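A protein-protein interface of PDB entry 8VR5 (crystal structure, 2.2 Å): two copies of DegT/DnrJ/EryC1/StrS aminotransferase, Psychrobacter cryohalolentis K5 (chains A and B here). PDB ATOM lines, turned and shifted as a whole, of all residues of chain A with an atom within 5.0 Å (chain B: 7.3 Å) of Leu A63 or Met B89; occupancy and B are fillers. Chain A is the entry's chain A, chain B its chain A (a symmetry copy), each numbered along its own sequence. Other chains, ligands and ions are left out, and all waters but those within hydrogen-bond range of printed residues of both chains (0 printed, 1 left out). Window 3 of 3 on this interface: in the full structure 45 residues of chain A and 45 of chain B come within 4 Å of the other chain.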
ATOM      1  N   HIS A  59      23.878  20.406 -23.899  1.00  0.00           N
ATOM      2  CA  HIS A  59      24.188  18.991 -24.038  1.00  0.00           C
ATOM      3  C   HIS A  59      23.080  18.293 -24.808  1.00  0.00           C
ATOM      4  O   HIS A  59      23.329  17.527 -25.749  1.00  0.00           O
ATOM      5  CB  HIS A  59      24.355  18.386 -22.653  1.00  0.00           C
ATOM      6  CG  HIS A  59      24.957  17.031 -22.585  1.00  0.00           C
ATOM      7  ND1 HIS A  59      25.148  16.432 -21.346  1.00  0.00           N
ATOM      8  CD2 HIS A  59      25.456  16.192 -23.533  1.00  0.00           C
ATOM      9  CE1 HIS A  59      25.733  15.256 -21.556  1.00  0.00           C
ATOM     10  NE2 HIS A  59      25.919  15.103 -22.864  1.00  0.00           N
ATOM     11  N   LEU A  60      21.838  18.575 -24.416  1.00  0.00           N
ATOM     12  CA  LEU A  60      20.686  17.950 -25.053  1.00  0.00           C
ATOM     13  C   LEU A  60      20.534  18.409 -26.492  1.00  0.00           C
ATOM     14  O   LEU A  60      20.053  17.645 -27.341  1.00  0.00           O
ATOM     15  CB  LEU A  60      19.430  18.257 -24.236  1.00  0.00           C
ATOM     16  CG  LEU A  60      19.374  17.535 -22.891  1.00  0.00           C
ATOM     17  CD1 LEU A  60      18.235  18.068 -22.063  1.00  0.00           C
ATOM     18  CD2 LEU A  60      19.231  16.026 -23.046  1.00  0.00           C
ATOM     19  N   ALA A  61      20.937  19.660 -26.747  1.00  0.00           N
ATOM     20  CA  ALA A  61      20.891  20.195 -28.100  1.00  0.00           C
ATOM     21  C   ALA A  61      21.864  19.399 -28.966  1.00  0.00           C
ATOM     22  O   ALA A  61      21.466  18.902 -30.018  1.00  0.00           O
ATOM     23  CB  ALA A  61      21.163  21.689 -28.121  1.00  0.00           C
ATOM     24  N   LEU A  62      23.094  19.198 -28.484  1.00  0.00           N
ATOM     25  CA  LEU A  62      24.062  18.373 -29.196  1.00  0.00           C
ATOM     26  C   LEU A  62      23.500  16.967 -29.417  1.00  0.00           C
ATOM     27  O   LEU A  62      23.513  16.470 -30.543  1.00  0.00           O
ATOM     28  CB  LEU A  62      25.392  18.348 -28.440  1.00  0.00           C
ATOM     29  CG  LEU A  62      26.118  19.691 -28.409  1.00  0.00           C
ATOM     30  CD1 LEU A  62      27.134  19.753 -27.284  1.00  0.00           C
ATOM     31  CD2 LEU A  62      26.813  19.986 -29.746  1.00  0.00           C
ATOM     32  N   LEU A  63      23.001  16.336 -28.354  1.00  0.00           N
ATOM     33  CA  LEU A  63      22.566  14.955 -28.433  1.00  0.00           C
ATOM     34  C   LEU A  63      21.359  14.858 -29.357  1.00  0.00           C
ATOM     35  O   LEU A  63      21.237  13.899 -30.085  1.00  0.00           O
ATOM     36  CB  LEU A  63      22.235  14.398 -27.037  1.00  0.00           C
ATOM     37  CG  LEU A  63      23.437  14.208 -26.109  1.00  0.00           C
ATOM     38  CD1 LEU A  63      23.000  13.837 -24.704  1.00  0.00           C
ATOM     39  CD2 LEU A  63      24.384  13.165 -26.676  1.00  0.00           C
ATOM     40  N   ALA A  64      20.459  15.824 -29.333  1.00  0.00           N
ATOM     41  CA  ALA A  64      19.274  15.705 -30.163  1.00  0.00           C
ATOM     42  C   ALA A  64      19.643  15.789 -31.650  1.00  0.00           C
ATOM     43  O   ALA A  64      18.944  15.244 -32.480  1.00  0.00           O
ATOM     44  CB  ALA A  64      18.245  16.742 -29.777  1.00  0.00           C
ATOM     45  N   LEU A  65      20.737  16.482 -31.982  1.00  0.00           N
ATOM     46  CA  LEU A  65      21.178  16.613 -33.363  1.00  0.00           C
ATOM     47  C   LEU A  65      22.115  15.467 -33.712  1.00  0.00           C
ATOM     48  O   LEU A  65      22.713  15.451 -34.775  1.00  0.00           O
ATOM     49  CB  LEU A  65      21.866  17.973 -33.524  1.00  0.00           C
ATOM     50  CG  LEU A  65      20.930  19.180 -33.506  1.00  0.00           C
ATOM     51  CD1 LEU A  65      21.679  20.475 -33.192  1.00  0.00           C
ATOM     52  CD2 LEU A  65      20.221  19.310 -34.844  1.00  0.00           C
ATOM     53  N   ASP A  66      22.277  14.531 -32.781  1.00  0.00           N
ATOM     54  CA  ASP A  66      23.132  13.387 -33.010  1.00  0.00           C
ATOM     55  C   ASP A  66      24.580  13.829 -33.266  1.00  0.00           C
ATOM     56  O   ASP A  66      25.240  13.313 -34.157  1.00  0.00           O
ATOM     57  CB  ASP A  66      22.554  12.539 -34.151  1.00  0.00           C
ATOM     58  CG  ASP A  66      23.225  11.186 -34.257  1.00  0.00           C
ATOM     59  OD1 ASP A  66      23.455  10.727 -35.399  1.00  0.00           O
ATOM     60  OD2 ASP A  66      23.552  10.615 -33.195  1.00  0.00           O
ATOM     61  N   ILE A  67      25.109  14.718 -32.419  1.00  0.00           N
ATOM     62  CA  ILE A  67      26.480  15.175 -32.547  1.00  0.00           C
ATOM     63  C   ILE A  67      27.334  14.469 -31.505  1.00  0.00           C
ATOM     64  O   ILE A  67      26.942  14.318 -30.354  1.00  0.00           O
ATOM     65  CB  ILE A  67      26.557  16.714 -32.488  1.00  0.00           C
ATOM     66  CG1 ILE A  67      25.891  17.344 -33.706  1.00  0.00           C
ATOM     67  CG2 ILE A  67      27.985  17.183 -32.364  1.00  0.00           C
ATOM     68  CD1 ILE A  67      25.652  18.849 -33.580  1.00  0.00           C
ATOM     69  N   THR A  90      30.567  15.121 -25.609  1.00  0.00           N
ATOM     70  CA  THR A  90      29.840  14.223 -26.493  1.00  0.00           C
ATOM     71  C   THR A  90      30.785  13.383 -27.350  1.00  0.00           C
ATOM     72  O   THR A  90      30.328  12.478 -28.018  1.00  0.00           O
ATOM     73  CB  THR A  90      28.908  14.947 -27.483  1.00  0.00           C
ATOM     74  OG1 THR A  90      29.707  15.700 -28.405  1.00  0.00           O
ATOM     75  CG2 THR A  90      27.899  15.851 -26.807  1.00  0.00           C
ATOM     76  N   LYS A 205      12.880  14.583 -29.244  1.00  0.00           N
ATOM     77  CA  LYS A 205      14.078  13.822 -28.927  1.00  0.00           C
ATOM     78  C   LYS A 205      14.751  14.363 -27.663  1.00  0.00           C
ATOM     79  O   LYS A 205      15.129  13.609 -26.789  1.00  0.00           O
ATOM     80  CB  LYS A 205      15.036  13.813 -30.125  1.00  0.00           C
ATOM     81  CG  LYS A 205      16.205  12.865 -29.953  1.00  0.00           C
ATOM     82  CD  LYS A 205      17.144  12.748 -31.119  1.00  0.00           C
ATOM     83  CE  LYS A 205      18.140  11.618 -30.907  1.00  0.00           C
ATOM     84  NZ  LYS A 205      19.279  11.677 -31.853  1.00  0.00           N
ATOM     85  N   LEU A 209      15.456  12.414 -24.110  1.00  0.00           N
ATOM     86  CA  LEU A 209      16.799  12.373 -23.549  1.00  0.00           C
ATOM     87  C   LEU A 209      16.830  12.972 -22.148  1.00  0.00           C
ATOM     88  O   LEU A 209      17.594  12.492 -21.312  1.00  0.00           O
ATOM     89  CB  LEU A 209      17.754  13.135 -24.464  1.00  0.00           C
ATOM     90  CG  LEU A 209      18.158  12.375 -25.723  1.00  0.00           C
ATOM     91  CD1 LEU A 209      19.060  13.232 -26.576  1.00  0.00           C
ATOM     92  CD2 LEU A 209      18.814  11.044 -25.392  1.00  0.00           C
ATOM     93  N   ILE A 226      17.432   5.104 -24.748  1.00  0.00           N
ATOM     94  CA  ILE A 226      18.289   5.461 -23.637  1.00  0.00           C
ATOM     95  C   ILE A 226      18.267   6.986 -23.465  1.00  0.00           C
ATOM     96  O   ILE A 226      18.141   7.741 -24.408  1.00  0.00           O
ATOM     97  CB  ILE A 226      19.709   4.888 -23.830  1.00  0.00           C
ATOM     98  CG1 ILE A 226      20.480   5.595 -24.943  1.00  0.00           C
ATOM     99  CG2 ILE A 226      19.639   3.393 -24.100  1.00  0.00           C
ATOM    100  CD1 ILE A 226      21.948   5.174 -25.041  1.00  0.00           C
ATOM    101  N   GLY A 227      18.359   7.455 -22.226  1.00  0.00           N
ATOM    102  CA  GLY A 227      18.458   8.879 -21.952  1.00  0.00           C
ATOM    103  C   GLY A 227      19.119   9.131 -20.599  1.00  0.00           C
ATOM    104  O   GLY A 227      19.700   8.214 -20.015  1.00  0.00           O
ATOM    105  N   LEU A 228      18.989  10.381 -20.143  1.00  0.00           N
ATOM    106  CA  LEU A 228      19.636  10.916 -18.955  1.00  0.00           C
ATOM    107  C   LEU A 228      18.567  11.402 -17.981  1.00  0.00           C
ATOM    108  O   LEU A 228      17.372  11.326 -18.255  1.00  0.00           O
ATOM    109  CB  LEU A 228      20.475  12.131 -19.383  1.00  0.00           C
ATOM    110  CG  LEU A 228      21.682  11.842 -20.257  1.00  0.00           C
ATOM    111  CD1 LEU A 228      22.259  13.126 -20.826  1.00  0.00           C
ATOM    112  CD2 LEU A 228      22.749  11.133 -19.458  1.00  0.00           C
ATOM    113  N   THR B  55      20.929   9.580 -11.263  1.00  0.00           N
ATOM    114  CA  THR B  55      21.488   9.217 -12.548  1.00  0.00           C
ATOM    115  C   THR B  55      22.832   9.927 -12.753  1.00  0.00           C
ATOM    116  O   THR B  55      23.789   9.343 -13.243  1.00  0.00           O
ATOM    117  CB  THR B  55      20.477   9.542 -13.661  1.00  0.00           C
ATOM    118  OG1 THR B  55      19.222   8.932 -13.340  1.00  0.00           O
ATOM    119  CG2 THR B  55      21.003   9.131 -15.030  1.00  0.00           C
ATOM    120  N   HIS B  59      26.503   8.411 -13.523  1.00  0.00           N
ATOM    121  CA  HIS B  59      27.186   8.893 -14.714  1.00  0.00           C
ATOM    122  C   HIS B  59      28.610   9.295 -14.366  1.00  0.00           C
ATOM    123  O   HIS B  59      29.573   8.921 -15.049  1.00  0.00           O
ATOM    124  CB  HIS B  59      26.410  10.071 -15.283  1.00  0.00           C
ATOM    125  CG  HIS B  59      26.779  10.513 -16.651  1.00  0.00           C
ATOM    126  ND1 HIS B  59      26.095  11.575 -17.231  1.00  0.00           N
ATOM    127  CD2 HIS B  59      27.670  10.045 -17.566  1.00  0.00           C
ATOM    128  CE1 HIS B  59      26.582  11.743 -18.457  1.00  0.00           C
ATOM    129  NE2 HIS B  59      27.528  10.832 -18.665  1.00  0.00           N
ATOM    130  N   LEU B  62      30.818   6.300 -13.667  1.00  0.00           N
ATOM    131  CA  LEU B  62      31.317   5.747 -14.920  1.00  0.00           C
ATOM    132  C   LEU B  62      32.453   6.613 -15.467  1.00  0.00           C
ATOM    133  O   LEU B  62      33.521   6.094 -15.790  1.00  0.00           O
ATOM    134  CB  LEU B  62      30.172   5.597 -15.924  1.00  0.00           C
ATOM    135  CG  LEU B  62      29.131   4.550 -15.534  1.00  0.00           C
ATOM    136  CD1 LEU B  62      27.817   4.768 -16.259  1.00  0.00           C
ATOM    137  CD2 LEU B  62      29.638   3.126 -15.806  1.00  0.00           C
ATOM    138  N   LEU B  63      32.228   7.924 -15.562  1.00  0.00           N
ATOM    139  CA  LEU B  63      33.190   8.809 -16.189  1.00  0.00           C
ATOM    140  C   LEU B  63      34.464   8.844 -15.354  1.00  0.00           C
ATOM    141  O   LEU B  63      35.540   8.907 -15.904  1.00  0.00           O
ATOM    142  CB  LEU B  63      32.610  10.224 -16.364  1.00  0.00           C
ATOM    143  CG  LEU B  63      31.482  10.344 -17.391  1.00  0.00           C
ATOM    144  CD1 LEU B  63      30.848  11.721 -17.361  1.00  0.00           C
ATOM    145  CD2 LEU B  63      31.996  10.013 -18.782  1.00  0.00           C
ATOM    146  N   ILE B  67      35.055   4.904 -18.106  1.00  0.00           N
ATOM    147  CA  ILE B  67      34.289   3.878 -18.790  1.00  0.00           C
ATOM    148  C   ILE B  67      33.501   4.521 -19.921  1.00  0.00           C
ATOM    149  O   ILE B  67      32.919   5.589 -19.766  1.00  0.00           O
ATOM    150  CB  ILE B  67      33.424   3.079 -17.794  1.00  0.00           C
ATOM    151  CG1 ILE B  67      34.293   2.258 -16.847  1.00  0.00           C
ATOM    152  CG2 ILE B  67      32.442   2.191 -18.515  1.00  0.00           C
ATOM    153  CD1 ILE B  67      33.541   1.684 -15.646  1.00  0.00           C
ATOM    154  N   GLY B  68      33.551   3.906 -21.104  1.00  0.00           N
ATOM    155  CA  GLY B  68      32.972   4.510 -22.292  1.00  0.00           C
ATOM    156  C   GLY B  68      32.980   3.540 -23.470  1.00  0.00           C
ATOM    157  O   GLY B  68      32.846   2.334 -23.272  1.00  0.00           O
ATOM    158  N   ALA B  82      17.357   3.765 -15.742  1.00  0.00           N
ATOM    159  CA  ALA B  82      18.533   4.619 -15.628  1.00  0.00           C
ATOM    160  C   ALA B  82      19.803   3.782 -15.486  1.00  0.00           C
ATOM    161  O   ALA B  82      20.841   4.142 -16.020  1.00  0.00           O
ATOM    162  CB  ALA B  82      18.365   5.564 -14.467  1.00  0.00           C
ATOM    163  N   ALA B  84      20.848   0.860 -16.638  1.00  0.00           N
ATOM    164  CA  ALA B  84      21.380   0.407 -17.913  1.00  0.00           C
ATOM    165  C   ALA B  84      21.577   1.576 -18.879  1.00  0.00           C
ATOM    166  O   ALA B  84      22.564   1.595 -19.602  1.00  0.00           O
ATOM    167  CB  ALA B  84      20.479  -0.628 -18.559  1.00  0.00           C
ATOM    168  N   ASN B  85      20.597   2.483 -18.960  1.00  0.00           N
ATOM    169  CA  ASN B  85      20.697   3.646 -19.816  1.00  0.00           C
ATOM    170  C   ASN B  85      22.008   4.366 -19.583  1.00  0.00           C
ATOM    171  O   ASN B  85      22.648   4.804 -20.539  1.00  0.00           O
ATOM    172  CB  ASN B  85      19.592   4.668 -19.572  1.00  0.00           C
ATOM    173  CG  ASN B  85      18.258   4.269 -20.162  1.00  0.00           C
ATOM    174  OD1 ASN B  85      18.171   3.335 -20.956  1.00  0.00           O
ATOM    175  ND2 ASN B  85      17.221   4.995 -19.803  1.00  0.00           N
ATOM    176  N   ILE B  86      22.371   4.585 -18.320  1.00  0.00           N
ATOM    177  CA  ILE B  86      23.441   5.549 -18.081  1.00  0.00           C
ATOM    178  C   ILE B  86      24.766   4.926 -18.525  1.00  0.00           C
ATOM    179  O   ILE B  86      25.632   5.620 -19.026  1.00  0.00           O
ATOM    180  CB  ILE B  86      23.461   6.071 -16.631  1.00  0.00           C
ATOM    181  CG1 ILE B  86      24.303   7.336 -16.502  1.00  0.00           C
ATOM    182  CG2 ILE B  86      23.950   5.001 -15.684  1.00  0.00           C
ATOM    183  CD1 ILE B  86      23.836   8.495 -17.341  1.00  0.00           C
ATOM    184  N   VAL B  87      24.884   3.613 -18.411  1.00  0.00           N
ATOM    185  CA  VAL B  87      26.025   2.905 -18.960  1.00  0.00           C
ATOM    186  C   VAL B  87      26.138   3.157 -20.463  1.00  0.00           C
ATOM    187  O   VAL B  87      27.215   3.459 -20.964  1.00  0.00           O
ATOM    188  CB  VAL B  87      25.899   1.405 -18.682  1.00  0.00           C
ATOM    189  CG1 VAL B  87      26.896   0.582 -19.490  1.00  0.00           C
ATOM    190  CG2 VAL B  87      26.018   1.103 -17.200  1.00  0.00           C
ATOM    191  N   GLU B  88      25.027   3.019 -21.191  1.00  0.00           N
ATOM    192  CA  GLU B  88      25.074   3.155 -22.633  1.00  0.00           C
ATOM    193  C   GLU B  88      25.261   4.614 -23.053  1.00  0.00           C
ATOM    194  O   GLU B  88      25.811   4.846 -24.127  1.00  0.00           O
ATOM    195  CB  GLU B  88      23.835   2.543 -23.284  1.00  0.00           C
ATOM    196  CG  GLU B  88      23.690   1.065 -22.984  1.00  0.00           C
ATOM    197  CD  GLU B  88      23.904   0.086 -24.129  1.00  0.00           C
ATOM    198  OE1 GLU B  88      23.829   0.501 -25.273  1.00  0.00           O
ATOM    199  OE2 GLU B  88      24.167  -1.087 -23.853  1.00  0.00           O
ATOM    200  N   MET B  89      24.853   5.593 -22.236  1.00  0.00           N
ATOM    201  CA  MET B  89      25.043   6.989 -22.619  1.00  0.00           C
ATOM    202  C   MET B  89      26.536   7.329 -22.670  1.00  0.00           C
ATOM    203  O   MET B  89      26.882   8.267 -23.375  1.00  0.00           O
ATOM    204  CB  MET B  89      24.360   7.973 -21.671  1.00  0.00           C
ATOM    205  CG  MET B  89      22.869   7.937 -21.781  1.00  0.00           C
ATOM    206  SD  MET B  89      22.271   8.470 -23.355  1.00  0.00           S
ATOM    207  CE  MET B  89      22.949  10.129 -23.423  1.00  0.00           C
ATOM    208  N   THR B  90      27.398   6.567 -21.971  1.00  0.00           N
ATOM    209  CA  THR B  90      28.833   6.800 -22.036  1.00  0.00           C
ATOM    210  C   THR B  90      29.455   6.167 -23.278  1.00  0.00           C
ATOM    211  O   THR B  90      30.613   6.413 -23.549  1.00  0.00           O
ATOM    212  CB  THR B  90      29.609   6.223 -20.837  1.00  0.00           C
ATOM    213  OG1 THR B  90      29.531   4.791 -20.881  1.00  0.00           O
ATOM    214  CG2 THR B  90      29.115   6.731 -19.499  1.00  0.00           C
ATOM    215  N   GLY B  91      28.732   5.307 -23.991  1.00  0.00           N
ATOM    216  CA  GLY B  91      29.320   4.553 -25.088  1.00  0.00           C
ATOM    217  C   GLY B  91      29.581   3.085 -24.749  1.00  0.00           C
ATOM    218  O   GLY B  91      29.733   2.267 -25.630  1.00  0.00           O
ATOM    219  N   ALA B  92      29.685   2.767 -23.461  1.00  0.00           N
ATOM    220  CA  ALA B  92      29.826   1.398 -23.017  1.00  0.00           C
ATOM    221  C   ALA B  92      28.557   0.606 -23.301  1.00  0.00           C
ATOM    222  O   ALA B  92      27.557   1.154 -23.705  1.00  0.00           O
ATOM    223  CB  ALA B  92      30.092   1.406 -21.539  1.00  0.00           C
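Leu A63 touches just one residue of chain B: Met B89 (3.9 Å). Of the printed residues of chain A, Glu B88 touches Ile A226. Of the printed residues of chain A, Asn B85 touches Ile A226 and Gly A227. Of the printed residues of chain B, Ile A226 touches Asn B85, Glu B88 and Met B89. Of the printed residues of chain B, Leu A228 touches Ile B86 and Met B89. Printed residues of chain A within 4 Å of Ile B86: Leu A228 (3.6 Å). Leu A209 touches none of the printed residues of chain B. Ala B92 touches none of the printed residues of chain A. The nearest printed residue of chain B that does not touch Leu A228 is His B59 (4.01 Å).
The side-chain amino group (NZ) of Lys A205 sits at hydrogen-bond distance from the backbone carbonyl oxygen (O) of Leu A63, at 3.4 Å. The backbone carbonyl oxygen (O) of Leu A209 sits at hydrogen-bond distance from the backbone NH (N) of Leu A228.
Hydrophobic or aromatic side chains of chain A within 4 Å of the printed part of chain B: Leu A63, Ile A226 and Leu A228. Hydrophobic or aromatic side chains of chain B that line the printed part of chain A: Ile B86 and Met B89.
Positions printed for both chains: 59, 62, 63, 67 and 90.
Met B89 touches Leu A63 (CE to CD1, 3.9 Å). OD1 of Asn B85 touches CA of Ile A226, 3.4 Å away. CD1 of Ile A226 touches CB of Glu B88 (3.7 Å). Met B89 touches Ile A226 (SD to CD1, 3.7 Å). O of Gly A227 touches CB of Asn B85, at 3.6 Å. Gly A227 touches Met B89 (O to CG, 3.6 Å). Leu A228 touches Ile B86 (CD2 to CD1, 3.6 Å). CG of Leu A228 touches CE of Met B89, 3.8 Å away.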
